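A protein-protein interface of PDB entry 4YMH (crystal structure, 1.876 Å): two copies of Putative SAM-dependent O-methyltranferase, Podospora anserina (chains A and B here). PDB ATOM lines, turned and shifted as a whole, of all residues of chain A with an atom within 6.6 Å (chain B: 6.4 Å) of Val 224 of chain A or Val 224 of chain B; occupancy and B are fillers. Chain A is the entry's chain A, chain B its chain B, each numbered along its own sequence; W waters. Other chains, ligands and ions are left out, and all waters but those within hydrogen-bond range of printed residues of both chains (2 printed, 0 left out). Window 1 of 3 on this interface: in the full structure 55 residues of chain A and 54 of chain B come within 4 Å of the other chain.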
ATOM      1  N   SER A   4     -13.812 -28.546 -28.255  1.00  0.00           N
ATOM      2  CA  SER A   4     -13.321 -29.349 -27.150  1.00  0.00           C
ATOM      3  C   SER A   4     -14.149 -29.275 -25.881  1.00  0.00           C
ATOM      4  O   SER A   4     -13.831 -29.952 -24.907  1.00  0.00           O
ATOM      5  CB  SER A   4     -11.891 -28.918 -26.821  1.00  0.00           C
ATOM      6  OG  SER A   4     -11.065 -29.077 -27.953  1.00  0.00           O
ATOM      7  N   TRP A  56      -7.768 -29.660  -6.739  1.00  0.00           N
ATOM      8  CA  TRP A  56      -6.861 -29.492  -7.880  1.00  0.00           C
ATOM      9  C   TRP A  56      -5.539 -28.838  -7.466  1.00  0.00           C
ATOM     10  O   TRP A  56      -4.465 -29.251  -7.899  1.00  0.00           O
ATOM     11  CB  TRP A  56      -7.552 -28.664  -8.969  1.00  0.00           C
ATOM     12  CG  TRP A  56      -6.647 -28.116 -10.022  1.00  0.00           C
ATOM     13  CD1 TRP A  56      -5.986 -28.819 -10.991  1.00  0.00           C
ATOM     14  CD2 TRP A  56      -6.332 -26.742 -10.240  1.00  0.00           C
ATOM     15  NE1 TRP A  56      -5.281 -27.963 -11.799  1.00  0.00           N
ATOM     16  CE2 TRP A  56      -5.470 -26.682 -11.356  1.00  0.00           C
ATOM     17  CE3 TRP A  56      -6.698 -25.549  -9.604  1.00  0.00           C
ATOM     18  CZ2 TRP A  56      -4.966 -25.483 -11.844  1.00  0.00           C
ATOM     19  CZ3 TRP A  56      -6.196 -24.357 -10.090  1.00  0.00           C
ATOM     20  CH2 TRP A  56      -5.339 -24.332 -11.200  1.00  0.00           C
ATOM     21  N   ASP A 172      -5.966 -17.722 -12.976  1.00  0.00           N
ATOM     22  CA  ASP A 172      -7.340 -18.138 -12.694  1.00  0.00           C
ATOM     23  C   ASP A 172      -8.392 -17.138 -13.206  1.00  0.00           C
ATOM     24  O   ASP A 172      -8.106 -15.950 -13.366  1.00  0.00           O
ATOM     25  CB  ASP A 172      -7.492 -18.342 -11.186  1.00  0.00           C
ATOM     26  CG  ASP A 172      -8.596 -19.297 -10.834  1.00  0.00           C
ATOM     27  OD1 ASP A 172      -8.894 -20.183 -11.657  1.00  0.00           O
ATOM     28  OD2 ASP A 172      -9.164 -19.168  -9.729  1.00  0.00           O
ATOM     29  N   PHE A 175     -11.588 -16.643 -18.127  1.00  0.00           N
ATOM     30  CA  PHE A 175     -12.789 -16.551 -18.966  1.00  0.00           C
ATOM     31  C   PHE A 175     -13.732 -15.423 -18.550  1.00  0.00           C
ATOM     32  O   PHE A 175     -14.604 -15.040 -19.323  1.00  0.00           O
ATOM     33  CB  PHE A 175     -13.587 -17.856 -18.926  1.00  0.00           C
ATOM     34  CG  PHE A 175     -12.997 -18.970 -19.758  1.00  0.00           C
ATOM     35  CD1 PHE A 175     -11.967 -18.729 -20.660  1.00  0.00           C
ATOM     36  CD2 PHE A 175     -13.494 -20.254 -19.646  1.00  0.00           C
ATOM     37  CE1 PHE A 175     -11.448 -19.764 -21.433  1.00  0.00           C
ATOM     38  CE2 PHE A 175     -12.968 -21.295 -20.411  1.00  0.00           C
ATOM     39  CZ  PHE A 175     -11.950 -21.047 -21.303  1.00  0.00           C
ATOM     40  N   LEU A 221      -4.447 -22.057 -22.824  1.00  0.00           N
ATOM     41  CA  LEU A 221      -5.656 -21.584 -22.167  1.00  0.00           C
ATOM     42  C   LEU A 221      -6.598 -22.761 -22.026  1.00  0.00           C
ATOM     43  O   LEU A 221      -7.259 -23.170 -22.977  1.00  0.00           O
ATOM     44  CB  LEU A 221      -6.298 -20.432 -22.951  1.00  0.00           C
ATOM     45  CG  LEU A 221      -7.590 -19.847 -22.359  1.00  0.00           C
ATOM     46  CD1 LEU A 221      -7.536 -19.692 -20.841  1.00  0.00           C
ATOM     47  CD2 LEU A 221      -7.951 -18.494 -23.036  1.00  0.00           C
ATOM     48  N   LEU A 222      -6.600 -23.327 -20.823  1.00  0.00           N
ATOM     49  CA  LEU A 222      -7.356 -24.527 -20.477  1.00  0.00           C
ATOM     50  C   LEU A 222      -8.804 -24.222 -20.108  1.00  0.00           C
ATOM     51  O   LEU A 222      -9.067 -23.446 -19.162  1.00  0.00           O
ATOM     52  CB  LEU A 222      -6.653 -25.231 -19.319  1.00  0.00           C
ATOM     53  CG  LEU A 222      -6.811 -26.741 -19.190  1.00  0.00           C
ATOM     54  CD1 LEU A 222      -6.328 -27.409 -20.462  1.00  0.00           C
ATOM     55  CD2 LEU A 222      -6.035 -27.237 -17.978  1.00  0.00           C
ATOM     56  N   PRO A 223      -9.760 -24.829 -20.843  1.00  0.00           N
ATOM     57  CA  PRO A 223     -11.177 -24.543 -20.588  1.00  0.00           C
ATOM     58  C   PRO A 223     -11.696 -25.359 -19.399  1.00  0.00           C
ATOM     59  O   PRO A 223     -12.562 -26.235 -19.548  1.00  0.00           O
ATOM     60  CB  PRO A 223     -11.864 -24.952 -21.895  1.00  0.00           C
ATOM     61  CG  PRO A 223     -11.007 -26.099 -22.393  1.00  0.00           C
ATOM     62  CD  PRO A 223      -9.576 -25.761 -21.977  1.00  0.00           C
ATOM     63  N   VAL A 224     -11.134 -25.069 -18.229  1.00  0.00           N
ATOM     64  CA  VAL A 224     -11.525 -25.734 -16.986  1.00  0.00           C
ATOM     65  C   VAL A 224     -11.839 -24.636 -15.955  1.00  0.00           C
ATOM     66  O   VAL A 224     -11.256 -23.563 -16.005  1.00  0.00           O
ATOM     67  CB  VAL A 224     -10.399 -26.697 -16.491  1.00  0.00           C
ATOM     68  CG1 VAL A 224      -9.204 -25.916 -15.949  1.00  0.00           C
ATOM     69  CG2 VAL A 224     -10.922 -27.747 -15.479  1.00  0.00           C
ATOM     70  N   PHE A 225     -12.766 -24.911 -15.040  1.00  0.00           N
ATOM     71  CA  PHE A 225     -13.177 -23.939 -14.023  1.00  0.00           C
ATOM     72  C   PHE A 225     -13.623 -22.646 -14.723  1.00  0.00           C
ATOM     73  O   PHE A 225     -14.437 -22.702 -15.636  1.00  0.00           O
ATOM     74  CB  PHE A 225     -12.040 -23.707 -13.018  1.00  0.00           C
ATOM     75  CG  PHE A 225     -11.559 -24.981 -12.345  1.00  0.00           C
ATOM     76  CD1 PHE A 225     -12.466 -25.869 -11.795  1.00  0.00           C
ATOM     77  CD2 PHE A 225     -10.208 -25.288 -12.267  1.00  0.00           C
ATOM     78  CE1 PHE A 225     -12.043 -27.038 -11.167  1.00  0.00           C
ATOM     79  CE2 PHE A 225      -9.783 -26.459 -11.636  1.00  0.00           C
ATOM     80  CZ  PHE A 225     -10.708 -27.333 -11.094  1.00  0.00           C
ATOM     81  N   ASP A 226     -13.089 -21.497 -14.321  1.00  0.00           N
ATOM     82  CA  ASP A 226     -13.471 -20.225 -14.951  1.00  0.00           C
ATOM     83  C   ASP A 226     -12.385 -19.805 -15.954  1.00  0.00           C
ATOM     84  O   ASP A 226     -12.163 -18.625 -16.206  1.00  0.00           O
ATOM     85  CB  ASP A 226     -13.701 -19.146 -13.876  1.00  0.00           C
ATOM     86  CG  ASP A 226     -14.350 -17.866 -14.428  1.00  0.00           C
ATOM     87  OD1 ASP A 226     -15.041 -17.914 -15.472  1.00  0.00           O
ATOM     88  OD2 ASP A 226     -14.163 -16.802 -13.793  1.00  0.00           O
ATOM     89  N   GLY A 227     -11.710 -20.798 -16.534  1.00  0.00           N
ATOM     90  CA  GLY A 227     -10.644 -20.547 -17.493  1.00  0.00           C
ATOM     91  C   GLY A 227      -9.308 -20.461 -16.777  1.00  0.00           C
ATOM     92  O   GLY A 227      -9.118 -19.606 -15.919  1.00  0.00           O
ATOM     93  N   VAL A 228      -8.378 -21.346 -17.129  1.00  0.00           N
ATOM     94  CA  VAL A 228      -7.069 -21.337 -16.477  1.00  0.00           C
ATOM     95  C   VAL A 228      -5.969 -21.245 -17.517  1.00  0.00           C
ATOM     96  O   VAL A 228      -5.810 -22.150 -18.332  1.00  0.00           O
ATOM     97  CB  VAL A 228      -6.852 -22.595 -15.626  1.00  0.00           C
ATOM     98  CG1 VAL A 228      -5.429 -22.608 -15.031  1.00  0.00           C
ATOM     99  CG2 VAL A 228      -7.937 -22.691 -14.532  1.00  0.00           C
ATOM    100  N   GLN A 230      -2.260 -21.616 -18.471  1.00  0.00           N
ATOM    101  CA  GLN A 230      -0.975 -22.206 -18.079  1.00  0.00           C
ATOM    102  C   GLN A 230       0.130 -21.547 -18.882  1.00  0.00           C
ATOM    103  O   GLN A 230       0.044 -21.453 -20.112  1.00  0.00           O
ATOM    104  CB  GLN A 230      -0.958 -23.728 -18.331  1.00  0.00           C
ATOM    105  CG  GLN A 230      -2.060 -24.473 -17.592  1.00  0.00           C
ATOM    106  CD  GLN A 230      -2.007 -25.976 -17.789  1.00  0.00           C
ATOM    107  OE1 GLN A 230      -1.215 -26.492 -18.576  1.00  0.00           O
ATOM    108  NE2 GLN A 230      -2.847 -26.686 -17.056  1.00  0.00           N
ATOM    109  N   SER B   4     -18.212 -25.741 -10.300  1.00  0.00           N
ATOM    110  CA  SER B   4     -16.936 -25.338 -10.866  1.00  0.00           C
ATOM    111  C   SER B   4     -16.940 -25.400 -12.383  1.00  0.00           C
ATOM    112  O   SER B   4     -15.895 -25.284 -13.014  1.00  0.00           O
ATOM    113  CB  SER B   4     -15.815 -26.222 -10.329  1.00  0.00           C
ATOM    114  OG  SER B   4     -15.744 -26.106  -8.935  1.00  0.00           O
ATOM    115  N   TRP B  56      -2.887 -29.289 -25.647  1.00  0.00           N
ATOM    116  CA  TRP B  56      -2.724 -29.711 -24.260  1.00  0.00           C
ATOM    117  C   TRP B  56      -1.721 -30.861 -24.100  1.00  0.00           C
ATOM    118  O   TRP B  56      -0.899 -30.847 -23.188  1.00  0.00           O
ATOM    119  CB  TRP B  56      -4.084 -30.113 -23.683  1.00  0.00           C
ATOM    120  CG  TRP B  56      -4.035 -30.869 -22.376  1.00  0.00           C
ATOM    121  CD1 TRP B  56      -3.756 -30.372 -21.130  1.00  0.00           C
ATOM    122  CD2 TRP B  56      -4.314 -32.253 -22.203  1.00  0.00           C
ATOM    123  NE1 TRP B  56      -3.832 -31.381 -20.191  1.00  0.00           N
ATOM    124  CE2 TRP B  56      -4.180 -32.543 -20.832  1.00  0.00           C
ATOM    125  CE3 TRP B  56      -4.660 -33.282 -23.085  1.00  0.00           C
ATOM    126  CZ2 TRP B  56      -4.372 -33.827 -20.325  1.00  0.00           C
ATOM    127  CZ3 TRP B  56      -4.847 -34.554 -22.582  1.00  0.00           C
ATOM    128  CH2 TRP B  56      -4.712 -34.812 -21.210  1.00  0.00           C
ATOM    129  N   ASP B 172      -8.755 -40.380 -20.486  1.00  0.00           N
ATOM    130  CA  ASP B 172      -9.516 -39.485 -21.355  1.00  0.00           C
ATOM    131  C   ASP B 172     -10.978 -39.898 -21.489  1.00  0.00           C
ATOM    132  O   ASP B 172     -11.312 -41.076 -21.323  1.00  0.00           O
ATOM    133  CB  ASP B 172      -8.868 -39.445 -22.739  1.00  0.00           C
ATOM    134  CG  ASP B 172      -9.135 -38.151 -23.475  1.00  0.00           C
ATOM    135  OD1 ASP B 172      -9.407 -37.119 -22.819  1.00  0.00           O
ATOM    136  OD2 ASP B 172      -9.043 -38.162 -24.715  1.00  0.00           O
ATOM    137  N   PHE B 175     -16.117 -38.531 -18.956  1.00  0.00           N
ATOM    138  CA  PHE B 175     -17.514 -38.083 -18.873  1.00  0.00           C
ATOM    139  C   PHE B 175     -18.470 -38.766 -19.855  1.00  0.00           C
ATOM    140  O   PHE B 175     -19.701 -38.677 -19.690  1.00  0.00           O
ATOM    141  CB  PHE B 175     -17.603 -36.582 -19.126  1.00  0.00           C
ATOM    142  CG  PHE B 175     -17.146 -35.727 -17.986  1.00  0.00           C
ATOM    143  CD1 PHE B 175     -16.871 -36.263 -16.744  1.00  0.00           C
ATOM    144  CD2 PHE B 175     -17.002 -34.358 -18.170  1.00  0.00           C
ATOM    145  CE1 PHE B 175     -16.455 -35.442 -15.691  1.00  0.00           C
ATOM    146  CE2 PHE B 175     -16.585 -33.535 -17.133  1.00  0.00           C
ATOM    147  CZ  PHE B 175     -16.315 -34.078 -15.890  1.00  0.00           C
ATOM    148  N   LEU B 222     -10.993 -34.015 -13.424  1.00  0.00           N
ATOM    149  CA  LEU B 222     -11.036 -32.611 -13.823  1.00  0.00           C
ATOM    150  C   LEU B 222     -12.063 -32.412 -14.934  1.00  0.00           C
ATOM    151  O   LEU B 222     -12.041 -33.157 -15.938  1.00  0.00           O
ATOM    152  CB  LEU B 222      -9.641 -32.163 -14.277  1.00  0.00           C
ATOM    153  CG  LEU B 222      -9.071 -30.812 -13.818  1.00  0.00           C
ATOM    154  CD1 LEU B 222      -9.434 -30.482 -12.374  1.00  0.00           C
ATOM    155  CD2 LEU B 222      -7.562 -30.784 -13.995  1.00  0.00           C
ATOM    156  N   PRO B 223     -12.969 -31.421 -14.756  1.00  0.00           N
ATOM    157  CA  PRO B 223     -14.026 -31.165 -15.731  1.00  0.00           C
ATOM    158  C   PRO B 223     -13.492 -30.351 -16.906  1.00  0.00           C
ATOM    159  O   PRO B 223     -13.872 -29.199 -17.079  1.00  0.00           O
ATOM    160  CB  PRO B 223     -15.068 -30.378 -14.926  1.00  0.00           C
ATOM    161  CG  PRO B 223     -14.267 -29.639 -13.922  1.00  0.00           C
ATOM    162  CD  PRO B 223     -13.101 -30.550 -13.570  1.00  0.00           C
ATOM    163  N   VAL B 224     -12.586 -30.948 -17.677  1.00  0.00           N
ATOM    164  CA  VAL B 224     -12.028 -30.299 -18.846  1.00  0.00           C
ATOM    165  C   VAL B 224     -12.180 -31.269 -20.017  1.00  0.00           C
ATOM    166  O   VAL B 224     -12.123 -32.485 -19.812  1.00  0.00           O
ATOM    167  CB  VAL B 224     -10.549 -29.895 -18.626  1.00  0.00           C
ATOM    168  CG1 VAL B 224      -9.629 -31.138 -18.527  1.00  0.00           C
ATOM    169  CG2 VAL B 224     -10.086 -28.931 -19.716  1.00  0.00           C
ATOM    170  N   PHE B 225     -12.402 -30.734 -21.221  1.00  0.00           N
ATOM    171  CA  PHE B 225     -12.588 -31.565 -22.414  1.00  0.00           C
ATOM    172  C   PHE B 225     -13.751 -32.530 -22.172  1.00  0.00           C
ATOM    173  O   PHE B 225     -14.829 -32.098 -21.756  1.00  0.00           O
ATOM    174  CB  PHE B 225     -11.284 -32.316 -22.752  1.00  0.00           C
ATOM    175  CG  PHE B 225     -10.096 -31.386 -22.980  1.00  0.00           C
ATOM    176  CD1 PHE B 225     -10.239 -30.247 -23.758  1.00  0.00           C
ATOM    177  CD2 PHE B 225      -8.866 -31.640 -22.386  1.00  0.00           C
ATOM    178  CE1 PHE B 225      -9.169 -29.387 -23.976  1.00  0.00           C
ATOM    179  CE2 PHE B 225      -7.787 -30.777 -22.603  1.00  0.00           C
ATOM    180  CZ  PHE B 225      -7.944 -29.656 -23.391  1.00  0.00           C
ATOM    181  N   ASP B 226     -13.531 -33.828 -22.401  1.00  0.00           N
ATOM    182  CA  ASP B 226     -14.585 -34.828 -22.189  1.00  0.00           C
ATOM    183  C   ASP B 226     -14.357 -35.529 -20.833  1.00  0.00           C
ATOM    184  O   ASP B 226     -14.768 -36.663 -20.625  1.00  0.00           O
ATOM    185  CB  ASP B 226     -14.604 -35.833 -23.350  1.00  0.00           C
ATOM    186  CG  ASP B 226     -15.858 -36.706 -23.381  1.00  0.00           C
ATOM    187  OD1 ASP B 226     -16.894 -36.306 -22.824  1.00  0.00           O
ATOM    188  OD2 ASP B 226     -15.800 -37.817 -23.975  1.00  0.00           O
ATOM    189  N   GLY B 227     -13.718 -34.815 -19.916  1.00  0.00           N
ATOM    190  CA  GLY B 227     -13.452 -35.331 -18.578  1.00  0.00           C
ATOM    191  C   GLY B 227     -12.088 -35.996 -18.550  1.00  0.00           C
ATOM    192  O   GLY B 227     -11.846 -36.930 -19.312  1.00  0.00           O
ATOM    193  N   VAL B 228     -11.194 -35.508 -17.692  1.00  0.00           N
ATOM    194  CA  VAL B 228      -9.854 -36.101 -17.622  1.00  0.00           C
ATOM    195  C   VAL B 228      -9.555 -36.500 -16.194  1.00  0.00           C
ATOM    196  O   VAL B 228      -9.550 -35.654 -15.310  1.00  0.00           O
ATOM    197  CB  VAL B 228      -8.745 -35.117 -18.105  1.00  0.00           C
ATOM    198  CG1 VAL B 228      -7.344 -35.785 -17.994  1.00  0.00           C
ATOM    199  CG2 VAL B 228      -9.013 -34.676 -19.528  1.00  0.00           C
ATOM    200  N   GLN B 230      -6.837 -37.618 -13.501  1.00  0.00           N
ATOM    201  CA  GLN B 230      -5.405 -37.687 -13.255  1.00  0.00           C
ATOM    202  C   GLN B 230      -5.193 -38.597 -12.053  1.00  0.00           C
ATOM    203  O   GLN B 230      -5.882 -38.464 -11.030  1.00  0.00           O
ATOM    204  CB  GLN B 230      -4.813 -36.289 -12.994  1.00  0.00           C
ATOM    205  CG  GLN B 230      -4.916 -35.345 -14.209  1.00  0.00           C
ATOM    206  CD  GLN B 230      -4.697 -33.877 -13.868  1.00  0.00           C
ATOM    207  OE1 GLN B 230      -4.444 -33.524 -12.724  1.00  0.00           O
ATOM    208  NE2 GLN B 230      -4.794 -33.012 -14.877  1.00  0.00           N
HETATM  209  O   HOH W   1     -14.805 -26.883 -15.819  1.00  0.00           O
HETATM  210  O   HOH W   2     -13.606 -28.089 -21.344  1.00  0.00           O
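Among the printed residues, merely in contact across the chains: Ser 4 of chain A with Phe 225 of chain B (3.2 Å), Trp 56 of chain A with Leu 222 of chain B (3.9 Å), Leu 222 of chain A with Trp 56 of chain B (3.98 Å), Leu 222 of chain A with Val 224 of chain B (3.97 Å), Pro 223 of chain A with Val 224 of chain B (3.7 Å), Val 224 of chain A with Leu 222 of chain B (3.9 Å), Val 224 of chain A with Pro 223 of chain B (3.7 Å), Val 224 of chain A with Val 224 of chain B (3.8 Å), Phe 225 of chain A with Ser 4 of chain B (3.2 Å) and Phe 225 of chain A with Leu 222 of chain B (3.6 Å).
N of Leu 222 of chain A lies within hydrogen-bond range of O of Val 228 of chain A (2.9 Å).
The backbone NH (N) of Leu 222 of chain B lies within hydrogen-bond range of the backbone carbonyl oxygen (O) of Val 228 of chain B.
Ser 4 of chain A touches Phe 225 of chain B, and with the chains exchanged Phe 225 of chain A touches Ser 4 of chain B.
Trp 56 of chain A touches Leu 222 of chain B, and with the chains exchanged Leu 222 of chain A touches Trp 56 of chain B.
Pro 223 of chain A touches Val 224 of chain B, and with the chains exchanged Val 224 of chain A touches Pro 223 of chain B.
Val 224 of chain B touches its own counterpart, Val 224 of chain A.
12 positions are printed for both chains.
Of the 10 pairs that touch across the chains among the printed residues, 9 have their exchanged pair printed and touching as well.
Val 224 of chain A touches just these residues of chain B: Leu 222, Pro 223 and Val 224.
Of chain A, only Leu 222, Pro 223 and Val 224 come within 4 Å of Val 224 of chain B.
Printed residues of chain B within 4 Å of Pro 223 of chain A: Val 224 (3.7 Å).
Of the printed residues of chain B, Ser 4 of chain A touches Phe 225 (3.2 Å).
The nearest residue of chain A that does not touch Val 224 of chain B is Ser 4 of chain A (5.3 Å).
The nearest printed residue of chain B that does not touch Phe 225 of chain A is Pro 223 of chain B (4.4 Å).
Water W2 bridges O of Pro 223 of chain A and N of Phe 225 of chain B.
Water W1 lies within hydrogen-bond range of the backbone carbonyl oxygen (O) of Pro 223 of chain B (2.8 Å), the backbone NH (N) of Phe 225 of chain A (2.9 Å) and the backbone carbonyl oxygen (O) of Ser 4 of chain B (3.4 Å).
Of the 13 printed residues of chain A, 6 touch a printed residue of chain B.
Hydrophobic or aromatic side chains of chain A that line the printed part of chain B: Trp 56, Leu 222, Pro 223, Val 224 and Phe 225.
Of the 12 printed residues of chain B, 6 touch a printed residue of chain A.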
